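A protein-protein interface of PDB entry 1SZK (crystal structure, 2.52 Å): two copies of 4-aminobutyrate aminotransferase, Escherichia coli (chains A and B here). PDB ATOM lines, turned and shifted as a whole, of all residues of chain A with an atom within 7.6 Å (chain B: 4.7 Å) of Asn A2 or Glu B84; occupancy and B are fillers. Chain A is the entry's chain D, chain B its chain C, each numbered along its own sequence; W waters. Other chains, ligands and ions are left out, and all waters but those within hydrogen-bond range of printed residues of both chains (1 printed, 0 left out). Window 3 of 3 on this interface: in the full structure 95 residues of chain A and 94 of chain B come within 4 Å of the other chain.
Asn A2 touches one residue of chain B.
Of the printed residues of chain B, Leu A7 touches Glu B84 and Leu B87.
Of the printed residues of chain B, Arg A10 touches Glu B84 (3.4 Å) and Leu B87 (3.7 Å).
Of the printed residues of chain B, Phe A26 touches Ala B82, Tyr B83, Glu B84 and Leu B87.
Of the printed residues of chain B, Ala A27 touches Ala B82 (2.6 Å) and Tyr B83 (3.9 Å).
Asp A28 touches none of the printed residues of chain B.
Of the printed residues of chain A, Ala B82 touches Phe A26 and Ala A27.
Of the printed residues of chain A, Glu B84 touches Asn A2 (3.8 Å), Leu A7 (3.9 Å), Arg A10 (3.4 Å) and Phe A26 (3.6 Å).
Glu B88 touches none of the printed residues of chain A.
The nearest printed residue of chain B that does not touch Asn A2 is Leu B87 (7.6 Å).
The side-chain amide oxygen of Asn A4 is in hydrogen-bond range of the backbone NH of Phe A26 (2.9 Å).
The backbone NH (N) of Val A38 sits at hydrogen-bond distance from the backbone carbonyl oxygen (O) of Phe A26 (3.0 Å).
OD1 of Asn A2 sits close to OE2 of Glu A6 (3.5 Å).
The backbone NH of Ala A27 lies within hydrogen-bond range of the backbone carbonyl oxygen of Ala B82, at 2.6 Å.
OE2 of Glu B84 lies within salt-bridge range of NH1 of Arg A10 (3.4 Å).
Water W1 lies within hydrogen-bond range of N of Glu B84 (2.5 Å) and O of Ala A27 (2.9 Å).
Among the printed residues, merely in contact across the chains: Asn A2 with Glu B84 (3.8 Å), Leu A7 with Glu B84 (3.9 Å), Leu A7 with Leu B87 (3.4 Å), Arg A10 with Leu B87 (3.7 Å), Phe A26 with Ala B82 (3.1 Å), Phe A26 with Tyr B83 (3.4 Å), Phe A26 with Glu B84 (3.6 Å), Phe A26 with Leu B87 (3.7 Å) and Ala A27 with Tyr B83 (3.9 Å).
No position is printed for both chains.
Of the 7 printed residues of chain B, 4 touch a printed residue of chain A.
Among the printed residues, 11 pairs touch across the chains.
Among the printed residues, Asp or Glu carboxylates within 4 Å of a Lys or Arg side-chain nitrogen of the other chain: Arg A10 with Glu B84 (3.4 Å).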
ATOM      1  N   ASN A   2     -24.519  22.273   6.484  1.00  0.00           N
ATOM      2  CA  ASN A   2     -23.118  22.013   6.027  1.00  0.00           C
ATOM      3  C   ASN A   2     -23.058  20.838   5.038  1.00  0.00           C
ATOM      4  O   ASN A   2     -24.086  20.406   4.506  1.00  0.00           O
ATOM      5  CB  ASN A   2     -22.218  21.721   7.233  1.00  0.00           C
ATOM      6  CG  ASN A   2     -20.828  22.342   7.098  1.00  0.00           C
ATOM      7  OD1 ASN A   2     -20.127  22.136   6.092  1.00  0.00           O
ATOM      8  ND2 ASN A   2     -20.417  23.101   8.119  1.00  0.00           N
ATOM      9  N   SER A   3     -21.849  20.331   4.800  1.00  0.00           N
ATOM     10  CA  SER A   3     -21.621  19.226   3.871  1.00  0.00           C
ATOM     11  C   SER A   3     -20.573  18.231   4.400  1.00  0.00           C
ATOM     12  O   SER A   3     -19.513  18.639   4.899  1.00  0.00           O
ATOM     13  CB  SER A   3     -21.153  19.799   2.519  1.00  0.00           C
ATOM     14  OG  SER A   3     -20.539  18.826   1.682  1.00  0.00           O
ATOM     15  N   ASN A   4     -20.859  16.934   4.291  1.00  0.00           N
ATOM     16  CA  ASN A   4     -19.904  15.924   4.725  1.00  0.00           C
ATOM     17  C   ASN A   4     -18.599  16.084   3.962  1.00  0.00           C
ATOM     18  O   ASN A   4     -17.514  16.137   4.553  1.00  0.00           O
ATOM     19  CB  ASN A   4     -20.444  14.515   4.490  1.00  0.00           C
ATOM     20  CG  ASN A   4     -21.458  14.097   5.536  1.00  0.00           C
ATOM     21  OD1 ASN A   4     -21.305  14.407   6.716  1.00  0.00           O
ATOM     22  ND2 ASN A   4     -22.489  13.374   5.113  1.00  0.00           N
ATOM     23  N   LYS A   5     -18.701  16.175   2.642  1.00  0.00           N
ATOM     24  CA  LYS A   5     -17.513  16.319   1.820  1.00  0.00           C
ATOM     25  C   LYS A   5     -16.762  17.605   2.122  1.00  0.00           C
ATOM     26  O   LYS A   5     -15.533  17.630   2.097  1.00  0.00           O
ATOM     27  CB  LYS A   5     -17.889  16.250   0.347  1.00  0.00           C
ATOM     28  CG  LYS A   5     -18.422  14.891  -0.087  1.00  0.00           C
ATOM     29  CD  LYS A   5     -18.890  14.942  -1.536  1.00  0.00           C
ATOM     30  CE  LYS A   5     -19.498  13.628  -1.970  1.00  0.00           C
ATOM     31  NZ  LYS A   5     -18.511  12.523  -1.864  1.00  0.00           N
ATOM     32  N   GLU A   6     -17.481  18.681   2.411  1.00  0.00           N
ATOM     33  CA  GLU A   6     -16.790  19.921   2.729  1.00  0.00           C
ATOM     34  C   GLU A   6     -16.011  19.765   4.032  1.00  0.00           C
ATOM     35  O   GLU A   6     -14.894  20.279   4.163  1.00  0.00           O
ATOM     36  CB  GLU A   6     -17.766  21.079   2.872  1.00  0.00           C
ATOM     37  CG  GLU A   6     -17.061  22.397   3.113  1.00  0.00           C
ATOM     38  CD  GLU A   6     -17.992  23.479   3.599  1.00  0.00           C
ATOM     39  OE1 GLU A   6     -19.042  23.708   2.954  1.00  0.00           O
ATOM     40  OE2 GLU A   6     -17.667  24.104   4.635  1.00  0.00           O
ATOM     41  N   LEU A   7     -16.600  19.062   5.002  1.00  0.00           N
ATOM     42  CA  LEU A   7     -15.929  18.834   6.281  1.00  0.00           C
ATOM     43  C   LEU A   7     -14.762  17.855   6.118  1.00  0.00           C
ATOM     44  O   LEU A   7     -13.748  17.983   6.798  1.00  0.00           O
ATOM     45  CB  LEU A   7     -16.930  18.347   7.339  1.00  0.00           C
ATOM     46  CG  LEU A   7     -17.909  19.461   7.761  1.00  0.00           C
ATOM     47  CD1 LEU A   7     -19.052  18.905   8.624  1.00  0.00           C
ATOM     48  CD2 LEU A   7     -17.134  20.553   8.492  1.00  0.00           C
ATOM     49  N   MET A   8     -14.894  16.894   5.208  1.00  0.00           N
ATOM     50  CA  MET A   8     -13.799  15.957   4.942  1.00  0.00           C
ATOM     51  C   MET A   8     -12.584  16.678   4.357  1.00  0.00           C
ATOM     52  O   MET A   8     -11.446  16.351   4.684  1.00  0.00           O
ATOM     53  CB  MET A   8     -14.238  14.860   3.980  1.00  0.00           C
ATOM     54  CG  MET A   8     -15.053  13.781   4.657  1.00  0.00           C
ATOM     55  SD  MET A   8     -14.089  12.991   5.976  1.00  0.00           S
ATOM     56  CE  MET A   8     -13.266  11.699   5.047  1.00  0.00           C
ATOM     57  N   ARG A  10     -11.658  19.764   4.926  1.00  0.00           N
ATOM     58  CA  ARG A  10     -10.994  20.525   5.979  1.00  0.00           C
ATOM     59  C   ARG A  10     -10.237  19.539   6.852  1.00  0.00           C
ATOM     60  O   ARG A  10      -9.125  19.817   7.296  1.00  0.00           O
ATOM     61  CB  ARG A  10     -12.021  21.295   6.809  1.00  0.00           C
ATOM     62  CG  ARG A  10     -12.761  22.351   6.004  1.00  0.00           C
ATOM     63  CD  ARG A  10     -13.961  22.878   6.746  1.00  0.00           C
ATOM     64  NE  ARG A  10     -13.595  23.489   8.013  1.00  0.00           N
ATOM     65  CZ  ARG A  10     -14.459  23.685   9.000  1.00  0.00           C
ATOM     66  NH1 ARG A  10     -15.728  23.315   8.855  1.00  0.00           N
ATOM     67  NH2 ARG A  10     -14.062  24.240  10.133  1.00  0.00           N
ATOM     68  N   PHE A  26     -19.828  13.222   8.855  1.00  0.00           N
ATOM     69  CA  PHE A  26     -19.731  13.945  10.105  1.00  0.00           C
ATOM     70  C   PHE A  26     -21.082  13.895  10.809  1.00  0.00           C
ATOM     71  O   PHE A  26     -22.097  14.342  10.276  1.00  0.00           O
ATOM     72  CB  PHE A  26     -19.318  15.398   9.872  1.00  0.00           C
ATOM     73  CG  PHE A  26     -17.837  15.591   9.721  1.00  0.00           C
ATOM     74  CD1 PHE A  26     -17.147  15.018   8.647  1.00  0.00           C
ATOM     75  CD2 PHE A  26     -17.133  16.362  10.636  1.00  0.00           C
ATOM     76  CE1 PHE A  26     -15.779  15.216   8.488  1.00  0.00           C
ATOM     77  CE2 PHE A  26     -15.757  16.570  10.490  1.00  0.00           C
ATOM     78  CZ  PHE A  26     -15.077  15.992   9.405  1.00  0.00           C
ATOM     79  N   ALA A  27     -21.090  13.339  12.009  1.00  0.00           N
ATOM     80  CA  ALA A  27     -22.314  13.241  12.781  1.00  0.00           C
ATOM     81  C   ALA A  27     -22.660  14.595  13.395  1.00  0.00           C
ATOM     82  O   ALA A  27     -21.780  15.425  13.643  1.00  0.00           O
ATOM     83  CB  ALA A  27     -22.151  12.189  13.870  1.00  0.00           C
ATOM     84  N   ASP A  28     -23.953  14.817  13.622  1.00  0.00           N
ATOM     85  CA  ASP A  28     -24.436  16.060  14.225  1.00  0.00           C
ATOM     86  C   ASP A  28     -25.177  15.755  15.534  1.00  0.00           C
ATOM     87  O   ASP A  28     -24.919  16.363  16.569  1.00  0.00           O
ATOM     88  CB  ASP A  28     -25.386  16.787  13.265  1.00  0.00           C
ATOM     89  CG  ASP A  28     -25.908  18.096  13.842  1.00  0.00           C
ATOM     90  OD1 ASP A  28     -25.066  18.959  14.182  1.00  0.00           O
ATOM     91  OD2 ASP A  28     -27.148  18.258  13.957  1.00  0.00           O
ATOM     92  N   ASP A  37     -26.326  13.038  10.230  1.00  0.00           N
ATOM     93  CA  ASP A  37     -25.130  13.776   9.820  1.00  0.00           C
ATOM     94  C   ASP A  37     -25.404  15.257   9.645  1.00  0.00           C
ATOM     95  O   ASP A  37     -26.531  15.710   9.790  1.00  0.00           O
ATOM     96  CB  ASP A  37     -24.530  13.216   8.516  1.00  0.00           C
ATOM     97  CG  ASP A  37     -25.528  13.174   7.359  1.00  0.00           C
ATOM     98  OD1 ASP A  37     -26.317  14.137   7.187  1.00  0.00           O
ATOM     99  OD2 ASP A  37     -25.504  12.168   6.612  1.00  0.00           O
ATOM    100  N   VAL A  38     -24.364  16.018   9.344  1.00  0.00           N
ATOM    101  CA  VAL A  38     -24.534  17.450   9.137  1.00  0.00           C
ATOM    102  C   VAL A  38     -25.464  17.754   7.949  1.00  0.00           C
ATOM    103  O   VAL A  38     -25.934  18.875   7.786  1.00  0.00           O
ATOM    104  CB  VAL A  38     -23.172  18.139   8.900  1.00  0.00           C
ATOM    105  CG1 VAL A  38     -22.357  18.119  10.182  1.00  0.00           C
ATOM    106  CG2 VAL A  38     -22.422  17.438   7.770  1.00  0.00           C
ATOM    107  N   GLU A  39     -25.739  16.750   7.126  1.00  0.00           N
ATOM    108  CA  GLU A  39     -26.609  16.957   5.974  1.00  0.00           C
ATOM    109  C   GLU A  39     -28.043  16.584   6.289  1.00  0.00           C
ATOM    110  O   GLU A  39     -28.924  16.670   5.431  1.00  0.00           O
ATOM    111  CB  GLU A  39     -26.087  16.167   4.767  1.00  0.00           C
ATOM    112  CG  GLU A  39     -24.874  16.830   4.110  1.00  0.00           C
ATOM    113  CD  GLU A  39     -24.300  16.035   2.943  1.00  0.00           C
ATOM    114  OE1 GLU A  39     -25.091  15.500   2.134  1.00  0.00           O
ATOM    115  OE2 GLU A  39     -23.054  15.958   2.821  1.00  0.00           O
ATOM    116  N   GLY A  40     -28.273  16.170   7.530  1.00  0.00           N
ATOM    117  CA  GLY A  40     -29.609  15.807   7.960  1.00  0.00           C
ATOM    118  C   GLY A  40     -29.994  14.371   7.698  1.00  0.00           C
ATOM    119  O   GLY A  40     -31.089  13.947   8.046  1.00  0.00           O
ATOM    120  N   ALA B  82     -16.930  11.081  12.068  1.00  0.00           N
ATOM    121  CA  ALA B  82     -16.375  12.345  12.527  1.00  0.00           C
ATOM    122  C   ALA B  82     -17.439  13.324  13.006  1.00  0.00           C
ATOM    123  O   ALA B  82     -18.641  13.082  12.867  1.00  0.00           O
ATOM    124  CB  ALA B  82     -15.545  12.985  11.426  1.00  0.00           C
ATOM    125  N   TYR B  83     -16.974  14.432  13.571  1.00  0.00           N
ATOM    126  CA  TYR B  83     -17.844  15.475  14.063  1.00  0.00           C
ATOM    127  C   TYR B  83     -17.057  16.764  14.052  1.00  0.00           C
ATOM    128  O   TYR B  83     -15.836  16.780  14.250  1.00  0.00           O
ATOM    129  CB  TYR B  83     -18.398  15.144  15.470  1.00  0.00           C
ATOM    130  CG  TYR B  83     -17.447  14.417  16.402  1.00  0.00           C
ATOM    131  CD1 TYR B  83     -16.561  15.124  17.206  1.00  0.00           C
ATOM    132  CD2 TYR B  83     -17.422  13.024  16.455  1.00  0.00           C
ATOM    133  CE1 TYR B  83     -15.680  14.471  18.035  1.00  0.00           C
ATOM    134  CE2 TYR B  83     -16.536  12.353  17.278  1.00  0.00           C
ATOM    135  CZ  TYR B  83     -15.661  13.083  18.068  1.00  0.00           C
ATOM    136  OH  TYR B  83     -14.740  12.450  18.884  1.00  0.00           O
ATOM    137  N   GLU B  84     -17.777  17.846  13.804  1.00  0.00           N
ATOM    138  CA  GLU B  84     -17.209  19.171  13.668  1.00  0.00           C
ATOM    139  C   GLU B  84     -16.402  19.758  14.814  1.00  0.00           C
ATOM    140  O   GLU B  84     -15.363  20.383  14.589  1.00  0.00           O
ATOM    141  CB  GLU B  84     -18.338  20.129  13.277  1.00  0.00           C
ATOM    142  CG  GLU B  84     -17.914  21.562  13.065  1.00  0.00           C
ATOM    143  CD  GLU B  84     -18.617  22.190  11.873  1.00  0.00           C
ATOM    144  OE1 GLU B  84     -19.740  21.725  11.544  1.00  0.00           O
ATOM    145  OE2 GLU B  84     -18.052  23.145  11.278  1.00  0.00           O
ATOM    146  N   PRO B  85     -16.857  19.572  16.057  1.00  0.00           N
ATOM    147  CA  PRO B  85     -16.083  20.150  17.158  1.00  0.00           C
ATOM    148  C   PRO B  85     -14.631  19.707  17.174  1.00  0.00           C
ATOM    149  O   PRO B  85     -13.751  20.481  17.527  1.00  0.00           O
ATOM    150  CB  PRO B  85     -16.857  19.703  18.400  1.00  0.00           C
ATOM    151  CG  PRO B  85     -18.270  19.573  17.887  1.00  0.00           C
ATOM    152  CD  PRO B  85     -18.053  18.877  16.561  1.00  0.00           C
ATOM    153  N   TYR B  86     -14.380  18.462  16.794  1.00  0.00           N
ATOM    154  CA  TYR B  86     -13.017  17.929  16.765  1.00  0.00           C
ATOM    155  C   TYR B  86     -12.229  18.644  15.655  1.00  0.00           C
ATOM    156  O   TYR B  86     -11.135  19.172  15.882  1.00  0.00           O
ATOM    157  CB  TYR B  86     -13.072  16.408  16.520  1.00  0.00           C
ATOM    158  CG  TYR B  86     -11.740  15.681  16.465  1.00  0.00           C
ATOM    159  CD1 TYR B  86     -11.581  14.452  17.114  1.00  0.00           C
ATOM    160  CD2 TYR B  86     -10.663  16.174  15.717  1.00  0.00           C
ATOM    161  CE1 TYR B  86     -10.396  13.732  17.022  1.00  0.00           C
ATOM    162  CE2 TYR B  86      -9.461  15.454  15.618  1.00  0.00           C
ATOM    163  CZ  TYR B  86      -9.342  14.235  16.278  1.00  0.00           C
ATOM    164  OH  TYR B  86      -8.174  13.514  16.225  1.00  0.00           O
ATOM    165  N   LEU B  87     -12.813  18.659  14.461  1.00  0.00           N
ATOM    166  CA  LEU B  87     -12.220  19.303  13.294  1.00  0.00           C
ATOM    167  C   LEU B  87     -11.922  20.773  13.566  1.00  0.00           C
ATOM    168  O   LEU B  87     -10.826  21.263  13.269  1.00  0.00           O
ATOM    169  CB  LEU B  87     -13.178  19.180  12.097  1.00  0.00           C
ATOM    170  CG  LEU B  87     -12.918  20.029  10.843  1.00  0.00           C
ATOM    171  CD1 LEU B  87     -11.506  19.831  10.346  1.00  0.00           C
ATOM    172  CD2 LEU B  87     -13.906  19.649   9.764  1.00  0.00           C
ATOM    173  N   GLU B  88     -12.901  21.466  14.138  1.00  0.00           N
ATOM    174  CA  GLU B  88     -12.755  22.891  14.424  1.00  0.00           C
ATOM    175  C   GLU B  88     -11.604  23.219  15.370  1.00  0.00           C
ATOM    176  O   GLU B  88     -10.806  24.125  15.100  1.00  0.00           O
ATOM    177  CB  GLU B  88     -14.060  23.461  14.993  1.00  0.00           C
ATOM    178  CG  GLU B  88     -14.082  24.980  15.035  1.00  0.00           C
ATOM    179  CD  GLU B  88     -15.382  25.545  15.588  1.00  0.00           C
ATOM    180  OE1 GLU B  88     -16.433  24.881  15.441  1.00  0.00           O
ATOM    181  OE2 GLU B  88     -15.353  26.663  16.155  1.00  0.00           O
HETATM  182  O   HOH W   1     -20.162  17.738  12.912  1.00  0.00           O
